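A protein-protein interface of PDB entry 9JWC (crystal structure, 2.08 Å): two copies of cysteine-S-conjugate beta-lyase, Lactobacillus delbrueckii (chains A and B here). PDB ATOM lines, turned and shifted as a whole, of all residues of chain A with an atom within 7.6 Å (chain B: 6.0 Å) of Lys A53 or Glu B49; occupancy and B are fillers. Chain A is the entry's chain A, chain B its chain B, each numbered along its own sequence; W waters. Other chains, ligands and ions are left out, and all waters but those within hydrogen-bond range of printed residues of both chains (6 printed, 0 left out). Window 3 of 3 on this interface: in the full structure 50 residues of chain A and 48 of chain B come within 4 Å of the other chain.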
ATOM      1  N   GLN A  15       2.927 -17.754   3.913  1.00  0.00           N
ATOM      2  CA  GLN A  15       3.675 -17.178   2.812  1.00  0.00           C
ATOM      3  C   GLN A  15       2.737 -16.943   1.624  1.00  0.00           C
ATOM      4  O   GLN A  15       1.567 -17.337   1.632  1.00  0.00           O
ATOM      5  CB  GLN A  15       4.849 -18.081   2.433  1.00  0.00           C
ATOM      6  CG  GLN A  15       5.792 -18.391   3.605  1.00  0.00           C
ATOM      7  CD  GLN A  15       7.149 -18.889   3.142  1.00  0.00           C
ATOM      8  OE1 GLN A  15       7.293 -19.363   2.011  1.00  0.00           O
ATOM      9  NE2 GLN A  15       8.151 -18.787   4.012  1.00  0.00           N
ATOM     10  N   MET A  45       5.058 -29.672  15.391  1.00  0.00           N
ATOM     11  CA  MET A  45       6.077 -28.699  15.021  1.00  0.00           C
ATOM     12  C   MET A  45       7.444 -29.122  15.543  1.00  0.00           C
ATOM     13  O   MET A  45       8.442 -29.061  14.814  1.00  0.00           O
ATOM     14  CB  MET A  45       5.672 -27.328  15.567  1.00  0.00           C
ATOM     15  CG  MET A  45       6.414 -26.146  14.994  1.00  0.00           C
ATOM     16  SD  MET A  45       6.048 -25.894  13.241  1.00  0.00           S
ATOM     17  CE  MET A  45       7.479 -26.719  12.583  1.00  0.00           C
ATOM     18  N   THR A  46       7.494 -29.579  16.800  1.00  0.00           N
ATOM     19  CA  THR A  46       8.741 -30.028  17.414  1.00  0.00           C
ATOM     20  C   THR A  46       9.410 -31.114  16.580  1.00  0.00           C
ATOM     21  O   THR A  46      10.622 -31.073  16.333  1.00  0.00           O
ATOM     22  CB  THR A  46       8.463 -30.541  18.830  1.00  0.00           C
ATOM     23  OG1 THR A  46       7.980 -29.468  19.640  1.00  0.00           O
ATOM     24  CG2 THR A  46       9.722 -31.093  19.468  1.00  0.00           C
ATOM     25  N   SER A  47       8.628 -32.093  16.124  1.00  0.00           N
ATOM     26  CA  SER A  47       9.209 -33.176  15.336  1.00  0.00           C
ATOM     27  C   SER A  47       9.691 -32.695  13.975  1.00  0.00           C
ATOM     28  O   SER A  47      10.686 -33.211  13.459  1.00  0.00           O
ATOM     29  CB  SER A  47       8.200 -34.307  15.149  1.00  0.00           C
ATOM     30  OG  SER A  47       7.239 -33.947  14.171  1.00  0.00           O
ATOM     31  N   MET A  48       9.001 -31.727  13.368  1.00  0.00           N
ATOM     32  CA  MET A  48       9.467 -31.200  12.087  1.00  0.00           C
ATOM     33  C   MET A  48      10.769 -30.438  12.260  1.00  0.00           C
ATOM     34  O   MET A  48      11.700 -30.589  11.460  1.00  0.00           O
ATOM     35  CB  MET A  48       8.418 -30.284  11.468  1.00  0.00           C
ATOM     36  CG  MET A  48       7.129 -30.955  11.086  1.00  0.00           C
ATOM     37  SD  MET A  48       6.018 -29.660  10.520  1.00  0.00           S
ATOM     38  CE  MET A  48       4.671 -30.647   9.877  1.00  0.00           C
ATOM     39  N   GLU A  49      10.831 -29.588  13.292  1.00  0.00           N
ATOM     40  CA  GLU A  49      12.027 -28.793  13.540  1.00  0.00           C
ATOM     41  C   GLU A  49      13.238 -29.686  13.766  1.00  0.00           C
ATOM     42  O   GLU A  49      14.327 -29.417  13.241  1.00  0.00           O
ATOM     43  CB  GLU A  49      11.794 -27.870  14.743  1.00  0.00           C
ATOM     44  CG  GLU A  49      10.986 -26.626  14.404  1.00  0.00           C
ATOM     45  CD  GLU A  49      10.402 -25.914  15.626  1.00  0.00           C
ATOM     46  OE1 GLU A  49      10.415 -26.488  16.737  1.00  0.00           O
ATOM     47  OE2 GLU A  49       9.906 -24.779  15.459  1.00  0.00           O
ATOM     48  N   GLU A  50      13.068 -30.758  14.539  1.00  0.00           N
ATOM     49  CA  GLU A  50      14.197 -31.641  14.823  1.00  0.00           C
ATOM     50  C   GLU A  50      14.606 -32.435  13.589  1.00  0.00           C
ATOM     51  O   GLU A  50      15.795 -32.711  13.392  1.00  0.00           O
ATOM     52  CB  GLU A  50      13.857 -32.585  15.978  1.00  0.00           C
ATOM     53  CG  GLU A  50      15.023 -33.487  16.378  1.00  0.00           C
ATOM     54  CD  GLU A  50      14.854 -34.109  17.746  1.00  0.00           C
ATOM     55  OE1 GLU A  50      15.886 -34.373  18.406  1.00  0.00           O
ATOM     56  OE2 GLU A  50      13.694 -34.329  18.163  1.00  0.00           O
ATOM     57  N   LYS A  51      13.640 -32.824  12.749  1.00  0.00           N
ATOM     58  CA  LYS A  51      13.989 -33.523  11.513  1.00  0.00           C
ATOM     59  C   LYS A  51      14.818 -32.630  10.595  1.00  0.00           C
ATOM     60  O   LYS A  51      15.759 -33.100   9.947  1.00  0.00           O
ATOM     61  CB  LYS A  51      12.723 -34.008  10.800  1.00  0.00           C
ATOM     62  CG  LYS A  51      12.984 -34.650   9.429  1.00  0.00           C
ATOM     63  CD  LYS A  51      13.935 -35.826   9.564  1.00  0.00           C
ATOM     64  CE  LYS A  51      14.194 -36.494   8.213  1.00  0.00           C
ATOM     65  NZ  LYS A  51      12.988 -37.257   7.728  1.00  0.00           N
ATOM     66  N   LEU A  52      14.484 -31.336  10.526  1.00  0.00           N
ATOM     67  CA  LEU A  52      15.244 -30.429   9.673  1.00  0.00           C
ATOM     68  C   LEU A  52      16.689 -30.318  10.131  1.00  0.00           C
ATOM     69  O   LEU A  52      17.578 -30.039   9.319  1.00  0.00           O
ATOM     70  CB  LEU A  52      14.615 -29.036   9.658  1.00  0.00           C
ATOM     71  CG  LEU A  52      13.431 -28.785   8.732  1.00  0.00           C
ATOM     72  CD1 LEU A  52      13.333 -27.287   8.478  1.00  0.00           C
ATOM     73  CD2 LEU A  52      13.564 -29.568   7.429  1.00  0.00           C
ATOM     74  N   LYS A  53      16.939 -30.511  11.428  1.00  0.00           N
ATOM     75  CA  LYS A  53      18.299 -30.420  11.942  1.00  0.00           C
ATOM     76  C   LYS A  53      19.211 -31.507  11.392  1.00  0.00           C
ATOM     77  O   LYS A  53      20.436 -31.367  11.498  1.00  0.00           O
ATOM     78  CB  LYS A  53      18.285 -30.480  13.464  1.00  0.00           C
ATOM     79  CG  LYS A  53      17.499 -29.336  14.117  1.00  0.00           C
ATOM     80  CD  LYS A  53      18.273 -28.042  14.033  1.00  0.00           C
ATOM     81  CE  LYS A  53      17.438 -26.834  14.430  1.00  0.00           C
ATOM     82  NZ  LYS A  53      18.178 -25.557  14.187  1.00  0.00           N
ATOM     83  N   VAL A  54      18.657 -32.590  10.833  1.00  0.00           N
ATOM     84  CA  VAL A  54      19.500 -33.572  10.147  1.00  0.00           C
ATOM     85  C   VAL A  54      20.370 -32.882   9.107  1.00  0.00           C
ATOM     86  O   VAL A  54      21.547 -33.223   8.933  1.00  0.00           O
ATOM     87  CB  VAL A  54      18.646 -34.690   9.513  1.00  0.00           C
ATOM     88  CG1 VAL A  54      19.537 -35.618   8.687  1.00  0.00           C
ATOM     89  CG2 VAL A  54      17.913 -35.485  10.583  1.00  0.00           C
ATOM     90  N   ALA A  55      19.817 -31.878   8.424  1.00  0.00           N
ATOM     91  CA  ALA A  55      20.548 -31.044   7.474  1.00  0.00           C
ATOM     92  C   ALA A  55      20.996 -31.821   6.237  1.00  0.00           C
ATOM     93  O   ALA A  55      21.955 -31.430   5.566  1.00  0.00           O
ATOM     94  CB  ALA A  55      21.754 -30.363   8.140  1.00  0.00           C
ATOM     95  N   ALA A  56      20.316 -32.919   5.936  1.00  0.00           N
ATOM     96  CA  ALA A  56      20.533 -33.700   4.727  1.00  0.00           C
ATOM     97  C   ALA A  56      19.286 -34.549   4.539  1.00  0.00           C
ATOM     98  O   ALA A  56      18.783 -35.139   5.499  1.00  0.00           O
ATOM     99  CB  ALA A  56      21.770 -34.596   4.813  1.00  0.00           C
ATOM    100  N   PHE A  57      18.781 -34.599   3.320  1.00  0.00           N
ATOM    101  CA  PHE A  57      17.460 -35.167   3.099  1.00  0.00           C
ATOM    102  C   PHE A  57      17.503 -36.171   1.956  1.00  0.00           C
ATOM    103  O   PHE A  57      16.926 -35.979   0.887  1.00  0.00           O
ATOM    104  CB  PHE A  57      16.478 -34.045   2.909  1.00  0.00           C
ATOM    105  CG  PHE A  57      16.480 -33.127   4.086  1.00  0.00           C
ATOM    106  CD1 PHE A  57      15.993 -33.581   5.302  1.00  0.00           C
ATOM    107  CD2 PHE A  57      17.083 -31.889   4.025  1.00  0.00           C
ATOM    108  CE1 PHE A  57      16.041 -32.777   6.414  1.00  0.00           C
ATOM    109  CE2 PHE A  57      17.133 -31.071   5.138  1.00  0.00           C
ATOM    110  CZ  PHE A  57      16.614 -31.520   6.332  1.00  0.00           C
ATOM    111  N   LYS B  13      24.019 -36.848  10.694  1.00  0.00           N
ATOM    112  CA  LYS B  13      23.516 -37.981  11.458  1.00  0.00           C
ATOM    113  C   LYS B  13      22.020 -38.109  11.181  1.00  0.00           C
ATOM    114  O   LYS B  13      21.229 -37.247  11.573  1.00  0.00           O
ATOM    115  CB  LYS B  13      23.821 -37.819  12.943  1.00  0.00           C
ATOM    116  CG  LYS B  13      25.323 -37.646  13.233  1.00  0.00           C
ATOM    117  CD  LYS B  13      26.050 -38.994  13.350  1.00  0.00           C
ATOM    118  CE  LYS B  13      27.523 -38.808  13.694  1.00  0.00           C
ATOM    119  NZ  LYS B  13      28.340 -38.585  12.463  1.00  0.00           N
ATOM    120  N   ARG B  39      26.156 -32.191   4.638  1.00  0.00           N
ATOM    121  CA  ARG B  39      25.062 -31.306   4.992  1.00  0.00           C
ATOM    122  C   ARG B  39      24.695 -30.449   3.793  1.00  0.00           C
ATOM    123  O   ARG B  39      25.534 -30.143   2.944  1.00  0.00           O
ATOM    124  CB  ARG B  39      25.458 -30.401   6.157  1.00  0.00           C
ATOM    125  CG  ARG B  39      25.792 -31.124   7.436  1.00  0.00           C
ATOM    126  CD  ARG B  39      26.194 -30.128   8.506  1.00  0.00           C
ATOM    127  NE  ARG B  39      25.497 -28.851   8.304  1.00  0.00           N
ATOM    128  CZ  ARG B  39      24.524 -28.399   9.092  1.00  0.00           C
ATOM    129  NH1 ARG B  39      24.132 -29.113  10.142  1.00  0.00           N
ATOM    130  NH2 ARG B  39      23.945 -27.242   8.832  1.00  0.00           N
ATOM    131  N   ILE B  44      19.792 -23.055   1.939  1.00  0.00           N
ATOM    132  CA  ILE B  44      18.579 -23.853   1.795  1.00  0.00           C
ATOM    133  C   ILE B  44      17.976 -24.144   3.162  1.00  0.00           C
ATOM    134  O   ILE B  44      16.763 -24.021   3.368  1.00  0.00           O
ATOM    135  CB  ILE B  44      18.876 -25.150   1.017  1.00  0.00           C
ATOM    136  CG1 ILE B  44      19.537 -24.831  -0.332  1.00  0.00           C
ATOM    137  CG2 ILE B  44      17.594 -25.982   0.832  1.00  0.00           C
ATOM    138  CD1 ILE B  44      20.076 -26.065  -1.073  1.00  0.00           C
ATOM    139  N   MET B  45      18.801 -24.543   4.113  1.00  0.00           N
ATOM    140  CA  MET B  45      18.275 -24.797   5.467  1.00  0.00           C
ATOM    141  C   MET B  45      17.507 -23.574   5.978  1.00  0.00           C
ATOM    142  O   MET B  45      16.423 -23.747   6.502  1.00  0.00           O
ATOM    143  CB  MET B  45      19.399 -25.166   6.439  1.00  0.00           C
ATOM    144  CG  MET B  45      18.944 -25.388   7.857  1.00  0.00           C
ATOM    145  SD  MET B  45      17.973 -26.893   8.024  1.00  0.00           S
ATOM    146  CE  MET B  45      18.901 -27.975   6.951  1.00  0.00           C
ATOM    147  N   THR B  46      18.094 -22.400   5.842  1.00  0.00           N
ATOM    148  CA  THR B  46      17.441 -21.194   6.338  1.00  0.00           C
ATOM    149  C   THR B  46      16.039 -21.049   5.761  1.00  0.00           C
ATOM    150  O   THR B  46      15.087 -20.727   6.482  1.00  0.00           O
ATOM    151  CB  THR B  46      18.284 -19.971   5.990  1.00  0.00           C
ATOM    152  OG1 THR B  46      19.471 -19.981   6.788  1.00  0.00           O
ATOM    153  CG2 THR B  46      17.503 -18.689   6.260  1.00  0.00           C
ATOM    154  N   SER B  47      15.894 -21.270   4.451  1.00  0.00           N
ATOM    155  CA  SER B  47      14.576 -21.125   3.843  1.00  0.00           C
ATOM    156  C   SER B  47      13.606 -22.179   4.352  1.00  0.00           C
ATOM    157  O   SER B  47      12.406 -21.921   4.428  1.00  0.00           O
ATOM    158  CB  SER B  47      14.664 -21.215   2.327  1.00  0.00           C
ATOM    159  OG  SER B  47      15.005 -22.544   1.948  1.00  0.00           O
ATOM    160  N   MET B  48      14.098 -23.373   4.688  1.00  0.00           N
ATOM    161  CA  MET B  48      13.213 -24.391   5.242  1.00  0.00           C
ATOM    162  C   MET B  48      12.780 -24.031   6.656  1.00  0.00           C
ATOM    163  O   MET B  48      11.611 -24.178   7.002  1.00  0.00           O
ATOM    164  CB  MET B  48      13.897 -25.753   5.223  1.00  0.00           C
ATOM    165  CG  MET B  48      14.099 -26.360   3.838  1.00  0.00           C
ATOM    166  SD  MET B  48      15.027 -27.892   4.106  1.00  0.00           S
ATOM    167  CE  MET B  48      15.094 -28.576   2.458  1.00  0.00           C
ATOM    168  N   GLU B  49      13.714 -23.571   7.497  1.00  0.00           N
ATOM    169  CA  GLU B  49      13.355 -23.169   8.857  1.00  0.00           C
ATOM    170  C   GLU B  49      12.451 -21.943   8.853  1.00  0.00           C
ATOM    171  O   GLU B  49      11.564 -21.831   9.706  1.00  0.00           O
ATOM    172  CB  GLU B  49      14.628 -22.920   9.682  1.00  0.00           C
ATOM    173  CG  GLU B  49      15.588 -24.089   9.603  1.00  0.00           C
ATOM    174  CD  GLU B  49      16.737 -24.047  10.595  1.00  0.00           C
ATOM    175  OE1 GLU B  49      16.888 -25.019  11.376  1.00  0.00           O
ATOM    176  OE2 GLU B  49      17.498 -23.063  10.575  1.00  0.00           O
ATOM    177  N   GLU B  50      12.669 -21.025   7.909  1.00  0.00           N
ATOM    178  CA  GLU B  50      11.763 -19.898   7.744  1.00  0.00           C
ATOM    179  C   GLU B  50      10.347 -20.374   7.423  1.00  0.00           C
ATOM    180  O   GLU B  50       9.374 -19.912   8.024  1.00  0.00           O
ATOM    181  CB  GLU B  50      12.283 -18.999   6.626  1.00  0.00           C
ATOM    182  CG  GLU B  50      11.407 -17.803   6.293  1.00  0.00           C
ATOM    183  CD  GLU B  50      11.237 -16.843   7.454  1.00  0.00           C
ATOM    184  OE1 GLU B  50      10.163 -16.201   7.534  1.00  0.00           O
ATOM    185  OE2 GLU B  50      12.179 -16.715   8.274  1.00  0.00           O
ATOM    186  N   LYS B  51      10.211 -21.316   6.488  1.00  0.00           N
ATOM    187  CA  LYS B  51       8.890 -21.794   6.087  1.00  0.00           C
ATOM    188  C   LYS B  51       8.166 -22.454   7.253  1.00  0.00           C
ATOM    189  O   LYS B  51       6.952 -22.283   7.415  1.00  0.00           O
ATOM    190  CB  LYS B  51       9.032 -22.754   4.891  1.00  0.00           C
ATOM    191  CG  LYS B  51       7.716 -23.375   4.430  1.00  0.00           C
ATOM    192  CD  LYS B  51       6.666 -22.326   4.113  1.00  0.00           C
ATOM    193  CE  LYS B  51       5.400 -22.975   3.538  1.00  0.00           C
ATOM    194  NZ  LYS B  51       5.626 -23.524   2.151  1.00  0.00           N
ATOM    195  N   LEU B  52       8.893 -23.193   8.090  1.00  0.00           N
ATOM    196  CA  LEU B  52       8.260 -23.891   9.208  1.00  0.00           C
ATOM    197  C   LEU B  52       7.597 -22.927  10.179  1.00  0.00           C
ATOM    198  O   LEU B  52       6.629 -23.296  10.858  1.00  0.00           O
ATOM    199  CB  LEU B  52       9.285 -24.739   9.950  1.00  0.00           C
ATOM    200  CG  LEU B  52       9.643 -26.096   9.356  1.00  0.00           C
ATOM    201  CD1 LEU B  52      10.334 -26.944  10.406  1.00  0.00           C
ATOM    202  CD2 LEU B  52       8.394 -26.816   8.810  1.00  0.00           C
ATOM    203  N   LYS B  53       8.105 -21.696  10.264  1.00  0.00           N
ATOM    204  CA  LYS B  53       7.555 -20.700  11.177  1.00  0.00           C
ATOM    205  C   LYS B  53       6.121 -20.328  10.834  1.00  0.00           C
ATOM    206  O   LYS B  53       5.423 -19.768  11.683  1.00  0.00           O
ATOM    207  CB  LYS B  53       8.431 -19.445  11.170  1.00  0.00           C
ATOM    208  CG  LYS B  53       9.894 -19.707  11.521  1.00  0.00           C
ATOM    209  CD  LYS B  53      10.036 -20.648  12.725  1.00  0.00           C
ATOM    210  CE  LYS B  53      11.502 -21.105  12.936  1.00  0.00           C
ATOM    211  NZ  LYS B  53      11.852 -22.410  12.239  1.00  0.00           N
ATOM    212  N   LEU B 271       7.620 -27.865   2.008  1.00  0.00           N
ATOM    213  CA  LEU B 271       8.949 -27.270   1.898  1.00  0.00           C
ATOM    214  C   LEU B 271       9.441 -27.136   0.464  1.00  0.00           C
ATOM    215  O   LEU B 271      10.425 -26.426   0.229  1.00  0.00           O
ATOM    216  CB  LEU B 271       9.961 -28.092   2.699  1.00  0.00           C
ATOM    217  CG  LEU B 271       9.745 -28.052   4.209  1.00  0.00           C
ATOM    218  CD1 LEU B 271      10.817 -28.910   4.881  1.00  0.00           C
ATOM    219  CD2 LEU B 271       9.776 -26.612   4.716  1.00  0.00           C
HETATM  220  O   HOH W   1      14.928 -26.972  12.428  1.00  0.00           O
HETATM  221  O   HOH W   2      10.868 -19.673   3.565  1.00  0.00           O
HETATM  222  O   HOH W   3      23.106 -33.754  11.027  1.00  0.00           O
HETATM  223  O   HOH W   4       6.001 -21.194   0.715  1.00  0.00           O
HETATM  224  O   HOH W   5       7.744 -17.764   6.816  1.00  0.00           O
HETATM  225  O   HOH W   6      21.847 -28.988  11.686  1.00  0.00           O
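Of the printed residues of chain B, Lys A53 touches Glu B49 (3.1 Å).
Of chain A, only Leu A52 and Lys A53 come within 4 Å of Glu B49.
Printed residues of chain A within 4 Å of Met B48: Leu A52 (3.6 Å) and Phe A57 (3.95 Å).
Of the printed residues of chain A, Arg B39 touches Ala A55 (3.2 Å).
Of the printed residues of chain B, Glu A49 touches Leu B52.
Printed residues of chain B within 4 Å of Ala A55: Arg B39 and Met B45.
Of the printed residues of chain B, Met A45 touches Leu B52 (3.6 Å).
Thr B46 touches none of the printed residues of chain A.
Lys A51 touches none of the printed residues of chain B.
The nearest residue of chain B that does not touch Lys A53 is Arg B39 (4.5 Å).
The nearest residue of chain A that does not touch Glu B49 is Glu A49 (5.4 Å).
Met A48 touches Leu B52, and with the chains exchanged Leu A52 touches Met B48.
Glu A49 touches Leu B52, and with the chains exchanged Leu A52 touches Glu B49.
Leu B52 touches its own counterpart, Leu A52.
Lys A53 touches Glu B49, but with the chains exchanged Glu A49 does not touch Lys B53 (4.4 Å).
Gln A15 touches Lys B51.
CD1 of Leu B52 touches N of Glu A49, 3.9 Å away.
Met B48 touches Leu A52.
Leu A52 touches Glu B49 (CD1 to N, 3.9 Å).
Leu A52 touches Leu B52 (CD1 to CD1, 3.6 Å).
Val A54 touches Lys B13.
Ala A55 touches Arg B39 (O to CA, 3.2 Å).
Met B45 touches Ala A55.
Phe A57 touches Met B45.
Phe A57 touches Met B48.
Water W4 lies within hydrogen-bond range of the side-chain amide oxygen of Gln A15 (2.6 Å) and the side-chain amino group of Lys B51 (2.8 Å).
Water W1 bridges the backbone carbonyl oxygen (O) of Glu A49 and the side-chain carboxylate (OE1) of Glu B49.
Water W3 lies within hydrogen-bond range of O of Val A54 and N of Lys B13.
Water W6 bridges NH1 of Arg B39 (2.8 Å) and O of Lys A53 (2.8 Å).
Water W2 lies within hydrogen-bond range of O of Ser B47, NE2 of Gln A15 and N of Lys B51.
Water W5 lies within hydrogen-bond range of O of Glu B50 (3.0 Å) and NE2 of Gln A15 (3.0 Å).
OE1 of Glu B49 lies within salt-bridge range of NZ of Lys A53.
SD of Met A45 sits close to O of Leu B52 (3.6 Å).
SD of Met B45 sits close to O of Leu A52 (3.4 Å).
Of the 14 printed residues of chain A, 9 touch a printed residue of chain B.
Printed residues of chain A that touch a printed residue of chain B: Gln A15, Met A45, Met A48, Glu A49, Leu A52, Lys A53, Val A54, Ala A55 and Phe A57.
Among the printed residues, 15 pairs touch across the chains.
Among the printed residues, Asp or Glu carboxylates within 4 Å of a Lys or Arg side-chain nitrogen of the other chain: Lys A53 with Glu B49 (3.1 Å).
The backbone carbonyl oxygen (O) of Glu B49 sits at hydrogen-bond distance from the side-chain amino group (NZ) of Lys B53, at 2.6 Å.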
